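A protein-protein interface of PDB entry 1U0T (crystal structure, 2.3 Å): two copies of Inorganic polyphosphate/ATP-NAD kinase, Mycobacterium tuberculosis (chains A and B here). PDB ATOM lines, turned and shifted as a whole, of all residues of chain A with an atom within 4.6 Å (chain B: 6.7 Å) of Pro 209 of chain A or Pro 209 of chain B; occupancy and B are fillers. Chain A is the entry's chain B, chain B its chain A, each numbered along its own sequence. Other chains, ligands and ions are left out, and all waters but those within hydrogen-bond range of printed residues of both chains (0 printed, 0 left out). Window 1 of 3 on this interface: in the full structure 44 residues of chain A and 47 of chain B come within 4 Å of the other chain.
The backbone carbonyl oxygen (O) of Val 210 of chain A sits at hydrogen-bond distance from the backbone NH (N) of Val 234 of chain B, 3.0 Å away.
The guanidinium group (NH1) of Arg 231 of chain B sits at hydrogen-bond distance from the backbone carbonyl oxygen (O) of Gly 208 of chain A (2.9 Å).
O of Pro 232 of chain B sits at hydrogen-bond distance from N of Val 210 of chain A (3.2 Å).
O of Val 210 of chain B is in hydrogen-bond range of N of Val 234 of chain A (2.9 Å).
The backbone carbonyl oxygen (O) of Pro 232 of chain A is in hydrogen-bond range of the backbone NH (N) of Val 210 of chain B (3.1 Å).
Of the 16 printed residues of chain B, 7 touch a printed residue of chain A.
Printed residues of chain B that touch a printed residue of chain A: Pro 209, Val 210, Leu 211, Arg 231, Pro 232, Met 233 and Val 234.
Hydrophobic or aromatic side chains of chain B within 4 Å of the printed part of chain A: Pro 209, Leu 211, Met 233 and Val 234.
Along chain B the printed residues that touch a printed residue of chain A span positions 209 to 234.
Of the 9 printed residues of chain A, 7 touch a printed residue of chain B.
Among the printed residues, merely in contact across the chains: Gly 207 of chain A with Arg 231 of chain B, Pro 209 of chain A with Pro 209 of chain B, Pro 209 of chain A with Pro 232 of chain B, Val 210 of chain A with Met 233 of chain B, Leu 211 of chain A with Val 234 of chain B, Pro 232 of chain A with Pro 209 of chain B and Val 234 of chain A with Leu 211 of chain B.
Printed residues of chain B within 4 Å of Gly 207 of chain A: Arg 231.
Of the printed residues of chain B, Gly 208 of chain A touches Arg 231 (2.9 Å).
Pro 209 of chain A touches just these residues of chain B: Pro 209 (3.9 Å) and Pro 232 (3.4 Å).
Of the printed residues of chain B, Val 234 of chain A touches Val 210 (2.9 Å) and Leu 211 (3.3 Å).
Gly 207 of chain B touches none of the printed residues of chain A.
Pro 209 of chain B touches two residues of chain A.
Leu 219 of chain B touches none of the printed residues of chain A.
Printed residues of chain A within 4 Å of Arg 231 of chain B: Gly 207 (3.4 Å) and Gly 208 (2.9 Å).
Printed residues of chain A within 4 Å of Pro 232 of chain B: Pro 209 and Val 210.
The nearest printed residue of chain A that does not touch Pro 209 of chain B is Val 234 of chain A (4.6 Å).
The nearest printed residue of chain B that does not touch Val 234 of chain A is Pro 209 of chain B (4.6 Å).
The side-chain hydroxyl of Ser 199 of chain B lies within hydrogen-bond range of the backbone NH of Leu 211 of chain B, 2.9 Å away.
The side-chain hydroxyl (OG) of Ser 199 of chain A sits at hydrogen-bond distance from the backbone NH (N) of Leu 211 of chain A (2.9 Å).
O of Met 233 of chain B sits at hydrogen-bond distance from N of Val 220 of chain B.
Pro 209 of chain B touches its own counterpart, Pro 209 of chain A.
Pro 209 of chain A touches Pro 232 of chain B, and with the chains exchanged Pro 232 of chain A touches Pro 209 of chain B.
Val 210 of chain A touches Val 234 of chain B, and with the chains exchanged Val 234 of chain A touches Val 210 of chain B.
Leu 211 of chain A touches Val 234 of chain B, and with the chains exchanged Val 234 of chain A touches Leu 211 of chain B.
Positions printed for both chains: 199, 207, 208, 209, 210, 211, 219, 232 and 234.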
ATOM      1  N   SER A 199      15.939  -3.347  26.554  1.00  0.00           N
ATOM      2  CA  SER A 199      14.871  -2.330  26.479  1.00  0.00           C
ATOM      3  C   SER A 199      13.607  -2.792  25.730  1.00  0.00           C
ATOM      4  O   SER A 199      12.516  -2.206  25.846  1.00  0.00           O
ATOM      5  CB  SER A 199      15.413  -1.023  25.906  1.00  0.00           C
ATOM      6  OG  SER A 199      15.647  -1.157  24.487  1.00  0.00           O
ATOM      7  N   GLY A 207       6.616  -0.009  29.991  1.00  0.00           N
ATOM      8  CA  GLY A 207       6.480   1.336  29.502  1.00  0.00           C
ATOM      9  C   GLY A 207       7.736   2.048  29.043  1.00  0.00           C
ATOM     10  O   GLY A 207       7.657   3.241  28.707  1.00  0.00           O
ATOM     11  N   GLY A 208       8.847   1.316  28.940  1.00  0.00           N
ATOM     12  CA  GLY A 208      10.114   1.883  28.522  1.00  0.00           C
ATOM     13  C   GLY A 208      10.220   2.360  27.079  1.00  0.00           C
ATOM     14  O   GLY A 208       9.496   1.907  26.211  1.00  0.00           O
ATOM     15  N   PRO A 209      11.175   3.260  26.828  1.00  0.00           N
ATOM     16  CA  PRO A 209      11.535   3.636  25.457  1.00  0.00           C
ATOM     17  C   PRO A 209      12.350   2.502  24.774  1.00  0.00           C
ATOM     18  O   PRO A 209      12.863   1.588  25.455  1.00  0.00           O
ATOM     19  CB  PRO A 209      12.405   4.895  25.635  1.00  0.00           C
ATOM     20  CG  PRO A 209      13.019   4.794  27.099  1.00  0.00           C
ATOM     21  CD  PRO A 209      11.989   3.952  27.860  1.00  0.00           C
ATOM     22  N   VAL A 210      12.420   2.540  23.446  1.00  0.00           N
ATOM     23  CA  VAL A 210      13.211   1.556  22.737  1.00  0.00           C
ATOM     24  C   VAL A 210      14.617   2.090  22.575  1.00  0.00           C
ATOM     25  O   VAL A 210      14.775   3.157  22.033  1.00  0.00           O
ATOM     26  CB  VAL A 210      12.605   1.226  21.337  1.00  0.00           C
ATOM     27  CG1 VAL A 210      13.472   0.167  20.644  1.00  0.00           C
ATOM     28  CG2 VAL A 210      11.146   0.731  21.494  1.00  0.00           C
ATOM     29  N   LEU A 211      15.632   1.390  23.087  1.00  0.00           N
ATOM     30  CA  LEU A 211      17.013   1.835  22.872  1.00  0.00           C
ATOM     31  C   LEU A 211      17.732   0.931  21.841  1.00  0.00           C
ATOM     32  O   LEU A 211      17.526  -0.277  21.837  1.00  0.00           O
ATOM     33  CB  LEU A 211      17.803   1.837  24.186  1.00  0.00           C
ATOM     34  CG  LEU A 211      17.621   2.966  25.238  1.00  0.00           C
ATOM     35  CD1 LEU A 211      16.146   3.287  25.600  1.00  0.00           C
ATOM     36  CD2 LEU A 211      18.385   2.552  26.505  1.00  0.00           C
ATOM     37  N   LEU A 219      19.129   2.169  31.565  1.00  0.00           N
ATOM     38  CA  LEU A 219      17.749   2.556  31.572  1.00  0.00           C
ATOM     39  C   LEU A 219      17.104   2.105  32.858  1.00  0.00           C
ATOM     40  O   LEU A 219      17.207   0.946  33.255  1.00  0.00           O
ATOM     41  CB  LEU A 219      17.007   1.957  30.364  1.00  0.00           C
ATOM     42  CG  LEU A 219      15.447   1.922  30.373  1.00  0.00           C
ATOM     43  CD1 LEU A 219      14.963   3.332  30.203  1.00  0.00           C
ATOM     44  CD2 LEU A 219      14.883   1.054  29.245  1.00  0.00           C
ATOM     45  N   PRO A 232      10.377   6.612  32.770  1.00  0.00           N
ATOM     46  CA  PRO A 232      11.689   6.014  32.515  1.00  0.00           C
ATOM     47  C   PRO A 232      12.758   7.067  32.550  1.00  0.00           C
ATOM     48  O   PRO A 232      12.511   8.215  32.228  1.00  0.00           O
ATOM     49  CB  PRO A 232      11.541   5.453  31.106  1.00  0.00           C
ATOM     50  CG  PRO A 232      10.030   5.213  30.977  1.00  0.00           C
ATOM     51  CD  PRO A 232       9.406   6.362  31.678  1.00  0.00           C
ATOM     52  N   VAL A 234      17.073   7.560  31.724  1.00  0.00           N
ATOM     53  CA  VAL A 234      18.219   7.014  31.024  1.00  0.00           C
ATOM     54  C   VAL A 234      19.457   7.803  31.415  1.00  0.00           C
ATOM     55  O   VAL A 234      19.462   9.037  31.439  1.00  0.00           O
ATOM     56  CB  VAL A 234      18.086   7.020  29.477  1.00  0.00           C
ATOM     57  CG1 VAL A 234      19.311   6.336  28.794  1.00  0.00           C
ATOM     58  CG2 VAL A 234      16.835   6.344  29.052  1.00  0.00           C
ATOM     59  N   SER B 199      15.857  16.916  26.965  1.00  0.00           N
ATOM     60  CA  SER B 199      14.891  15.901  27.392  1.00  0.00           C
ATOM     61  C   SER B 199      13.866  16.335  28.501  1.00  0.00           C
ATOM     62  O   SER B 199      12.768  15.744  28.597  1.00  0.00           O
ATOM     63  CB  SER B 199      15.601  14.577  27.739  1.00  0.00           C
ATOM     64  OG  SER B 199      16.060  14.562  29.101  1.00  0.00           O
ATOM     65  N   THR B 200      14.212  17.342  29.306  1.00  0.00           N
ATOM     66  CA  THR B 200      13.306  17.876  30.337  1.00  0.00           C
ATOM     67  C   THR B 200      12.371  18.950  29.759  1.00  0.00           C
ATOM     68  O   THR B 200      11.557  19.543  30.509  1.00  0.00           O
ATOM     69  CB  THR B 200      14.129  18.563  31.495  1.00  0.00           C
ATOM     70  OG1 THR B 200      15.114  19.430  30.918  1.00  0.00           O
ATOM     71  CG2 THR B 200      14.979  17.541  32.280  1.00  0.00           C
ATOM     72  N   ALA B 203      10.293  17.864  24.843  1.00  0.00           N
ATOM     73  CA  ALA B 203      10.340  16.413  24.692  1.00  0.00           C
ATOM     74  C   ALA B 203       9.647  15.690  25.841  1.00  0.00           C
ATOM     75  O   ALA B 203       8.928  14.723  25.605  1.00  0.00           O
ATOM     76  CB  ALA B 203      11.795  15.939  24.569  1.00  0.00           C
ATOM     77  N   PHE B 204       9.894  16.154  27.066  1.00  0.00           N
ATOM     78  CA  PHE B 204       9.179  15.723  28.234  1.00  0.00           C
ATOM     79  C   PHE B 204       7.651  15.866  28.154  1.00  0.00           C
ATOM     80  O   PHE B 204       6.934  14.921  28.515  1.00  0.00           O
ATOM     81  CB  PHE B 204       9.640  16.518  29.470  1.00  0.00           C
ATOM     82  CG  PHE B 204       9.041  16.015  30.743  1.00  0.00           C
ATOM     83  CD1 PHE B 204       9.584  14.930  31.390  1.00  0.00           C
ATOM     84  CD2 PHE B 204       7.907  16.593  31.265  1.00  0.00           C
ATOM     85  CE1 PHE B 204       9.013  14.421  32.560  1.00  0.00           C
ATOM     86  CE2 PHE B 204       7.334  16.098  32.435  1.00  0.00           C
ATOM     87  CZ  PHE B 204       7.889  15.004  33.082  1.00  0.00           C
ATOM     88  N   GLY B 207       5.996  13.267  26.086  1.00  0.00           N
ATOM     89  CA  GLY B 207       5.881  11.921  26.627  1.00  0.00           C
ATOM     90  C   GLY B 207       7.220  11.226  26.811  1.00  0.00           C
ATOM     91  O   GLY B 207       7.233  10.031  27.129  1.00  0.00           O
ATOM     92  N   GLY B 208       8.319  11.961  26.621  1.00  0.00           N
ATOM     93  CA  GLY B 208       9.650  11.361  26.642  1.00  0.00           C
ATOM     94  C   GLY B 208      10.227  11.069  28.014  1.00  0.00           C
ATOM     95  O   GLY B 208       9.755  11.599  29.019  1.00  0.00           O
ATOM     96  N   PRO B 209      11.231  10.197  28.048  1.00  0.00           N
ATOM     97  CA  PRO B 209      11.929   9.849  29.287  1.00  0.00           C
ATOM     98  C   PRO B 209      12.867  10.946  29.660  1.00  0.00           C
ATOM     99  O   PRO B 209      13.175  11.806  28.818  1.00  0.00           O
ATOM    100  CB  PRO B 209      12.782   8.614  28.907  1.00  0.00           C
ATOM    101  CG  PRO B 209      12.898   8.684  27.368  1.00  0.00           C
ATOM    102  CD  PRO B 209      11.729   9.441  26.880  1.00  0.00           C
ATOM    103  N   VAL B 210      13.387  10.873  30.879  1.00  0.00           N
ATOM    104  CA  VAL B 210      14.324  11.883  31.331  1.00  0.00           C
ATOM    105  C   VAL B 210      15.701  11.311  31.180  1.00  0.00           C
ATOM    106  O   VAL B 210      15.974  10.249  31.748  1.00  0.00           O
ATOM    107  CB  VAL B 210      14.137  12.211  32.832  1.00  0.00           C
ATOM    108  CG1 VAL B 210      15.272  13.055  33.307  1.00  0.00           C
ATOM    109  CG2 VAL B 210      12.689  12.843  33.128  1.00  0.00           C
ATOM    110  N   LEU B 211      16.566  12.046  30.476  1.00  0.00           N
ATOM    111  CA  LEU B 211      17.952  11.663  30.220  1.00  0.00           C
ATOM    112  C   LEU B 211      18.878  12.577  31.012  1.00  0.00           C
ATOM    113  O   LEU B 211      18.651  13.797  31.091  1.00  0.00           O
ATOM    114  CB  LEU B 211      18.272  11.802  28.722  1.00  0.00           C
ATOM    115  CG  LEU B 211      17.867  10.639  27.778  1.00  0.00           C
ATOM    116  CD1 LEU B 211      16.367  10.221  27.886  1.00  0.00           C
ATOM    117  CD2 LEU B 211      18.205  11.002  26.355  1.00  0.00           C
ATOM    118  N   LEU B 219      17.680  11.396  21.265  1.00  0.00           N
ATOM    119  CA  LEU B 219      16.343  10.995  21.691  1.00  0.00           C
ATOM    120  C   LEU B 219      15.338  11.439  20.637  1.00  0.00           C
ATOM    121  O   LEU B 219      15.373  12.591  20.206  1.00  0.00           O
ATOM    122  CB  LEU B 219      16.025  11.694  23.041  1.00  0.00           C
ATOM    123  CG  LEU B 219      14.546  11.716  23.467  1.00  0.00           C
ATOM    124  CD1 LEU B 219      13.953  10.263  23.700  1.00  0.00           C
ATOM    125  CD2 LEU B 219      14.306  12.617  24.696  1.00  0.00           C
ATOM    126  N   VAL B 220      14.477  10.537  20.198  1.00  0.00           N
ATOM    127  CA  VAL B 220      13.445  10.838  19.198  1.00  0.00           C
ATOM    128  C   VAL B 220      12.075  10.618  19.850  1.00  0.00           C
ATOM    129  O   VAL B 220      11.781   9.506  20.331  1.00  0.00           O
ATOM    130  CB  VAL B 220      13.577   9.900  17.973  1.00  0.00           C
ATOM    131  CG1 VAL B 220      12.666  10.334  16.816  1.00  0.00           C
ATOM    132  CG2 VAL B 220      15.046   9.840  17.476  1.00  0.00           C
ATOM    133  N   VAL B 221      11.243  11.658  19.895  1.00  0.00           N
ATOM    134  CA  VAL B 221       9.897  11.517  20.489  1.00  0.00           C
ATOM    135  C   VAL B 221       8.832  11.895  19.446  1.00  0.00           C
ATOM    136  O   VAL B 221       8.750  13.063  19.071  1.00  0.00           O
ATOM    137  CB  VAL B 221       9.727  12.456  21.759  1.00  0.00           C
ATOM    138  CG1 VAL B 221       8.334  12.320  22.388  1.00  0.00           C
ATOM    139  CG2 VAL B 221      10.786  12.168  22.768  1.00  0.00           C
ATOM    140  N   ARG B 231       6.145   5.278  20.636  1.00  0.00           N
ATOM    141  CA  ARG B 231       7.069   5.371  21.761  1.00  0.00           C
ATOM    142  C   ARG B 231       8.381   6.157  21.417  1.00  0.00           C
ATOM    143  O   ARG B 231       8.785   6.183  20.292  1.00  0.00           O
ATOM    144  CB  ARG B 231       7.400   3.945  22.176  1.00  0.00           C
ATOM    145  CG  ARG B 231       6.234   3.224  22.807  1.00  0.00           C
ATOM    146  CD  ARG B 231       6.717   2.216  23.759  1.00  0.00           C
ATOM    147  NE  ARG B 231       5.642   1.385  24.226  1.00  0.00           N
ATOM    148  CZ  ARG B 231       5.716   0.676  25.297  1.00  0.00           C
ATOM    149  NH1 ARG B 231       6.840   0.673  26.026  1.00  0.00           N
ATOM    150  NH2 ARG B 231       4.676  -0.064  25.639  1.00  0.00           N
ATOM    151  N   PRO B 232       9.008   6.824  22.386  1.00  0.00           N
ATOM    152  CA  PRO B 232      10.298   7.480  22.163  1.00  0.00           C
ATOM    153  C   PRO B 232      11.358   6.430  21.974  1.00  0.00           C
ATOM    154  O   PRO B 232      11.173   5.330  22.463  1.00  0.00           O
ATOM    155  CB  PRO B 232      10.550   8.199  23.489  1.00  0.00           C
ATOM    156  CG  PRO B 232       9.121   8.280  24.122  1.00  0.00           C
ATOM    157  CD  PRO B 232       8.533   7.002  23.772  1.00  0.00           C
ATOM    158  N   MET B 233      12.433   6.791  21.293  1.00  0.00           N
ATOM    159  CA  MET B 233      13.525   5.905  20.907  1.00  0.00           C
ATOM    160  C   MET B 233      14.841   6.650  21.207  1.00  0.00           C
ATOM    161  O   MET B 233      14.920   7.862  21.008  1.00  0.00           O
ATOM    162  CB  MET B 233      13.435   5.679  19.388  1.00  0.00           C
ATOM    163  CG  MET B 233      12.121   4.940  18.964  1.00  0.00           C
ATOM    164  SD  MET B 233      11.730   5.052  17.193  1.00  0.00           S
ATOM    165  CE  MET B 233      10.808   6.561  17.169  1.00  0.00           C
ATOM    166  N   VAL B 234      15.847   5.932  21.671  1.00  0.00           N
ATOM    167  CA  VAL B 234      17.082   6.525  22.042  1.00  0.00           C
ATOM    168  C   VAL B 234      18.185   5.745  21.328  1.00  0.00           C
ATOM    169  O   VAL B 234      18.265   4.535  21.405  1.00  0.00           O
ATOM    170  CB  VAL B 234      17.360   6.474  23.591  1.00  0.00           C
ATOM    171  CG1 VAL B 234      18.608   7.253  23.954  1.00  0.00           C
ATOM    172  CG2 VAL B 234      16.150   6.966  24.404  1.00  0.00           C
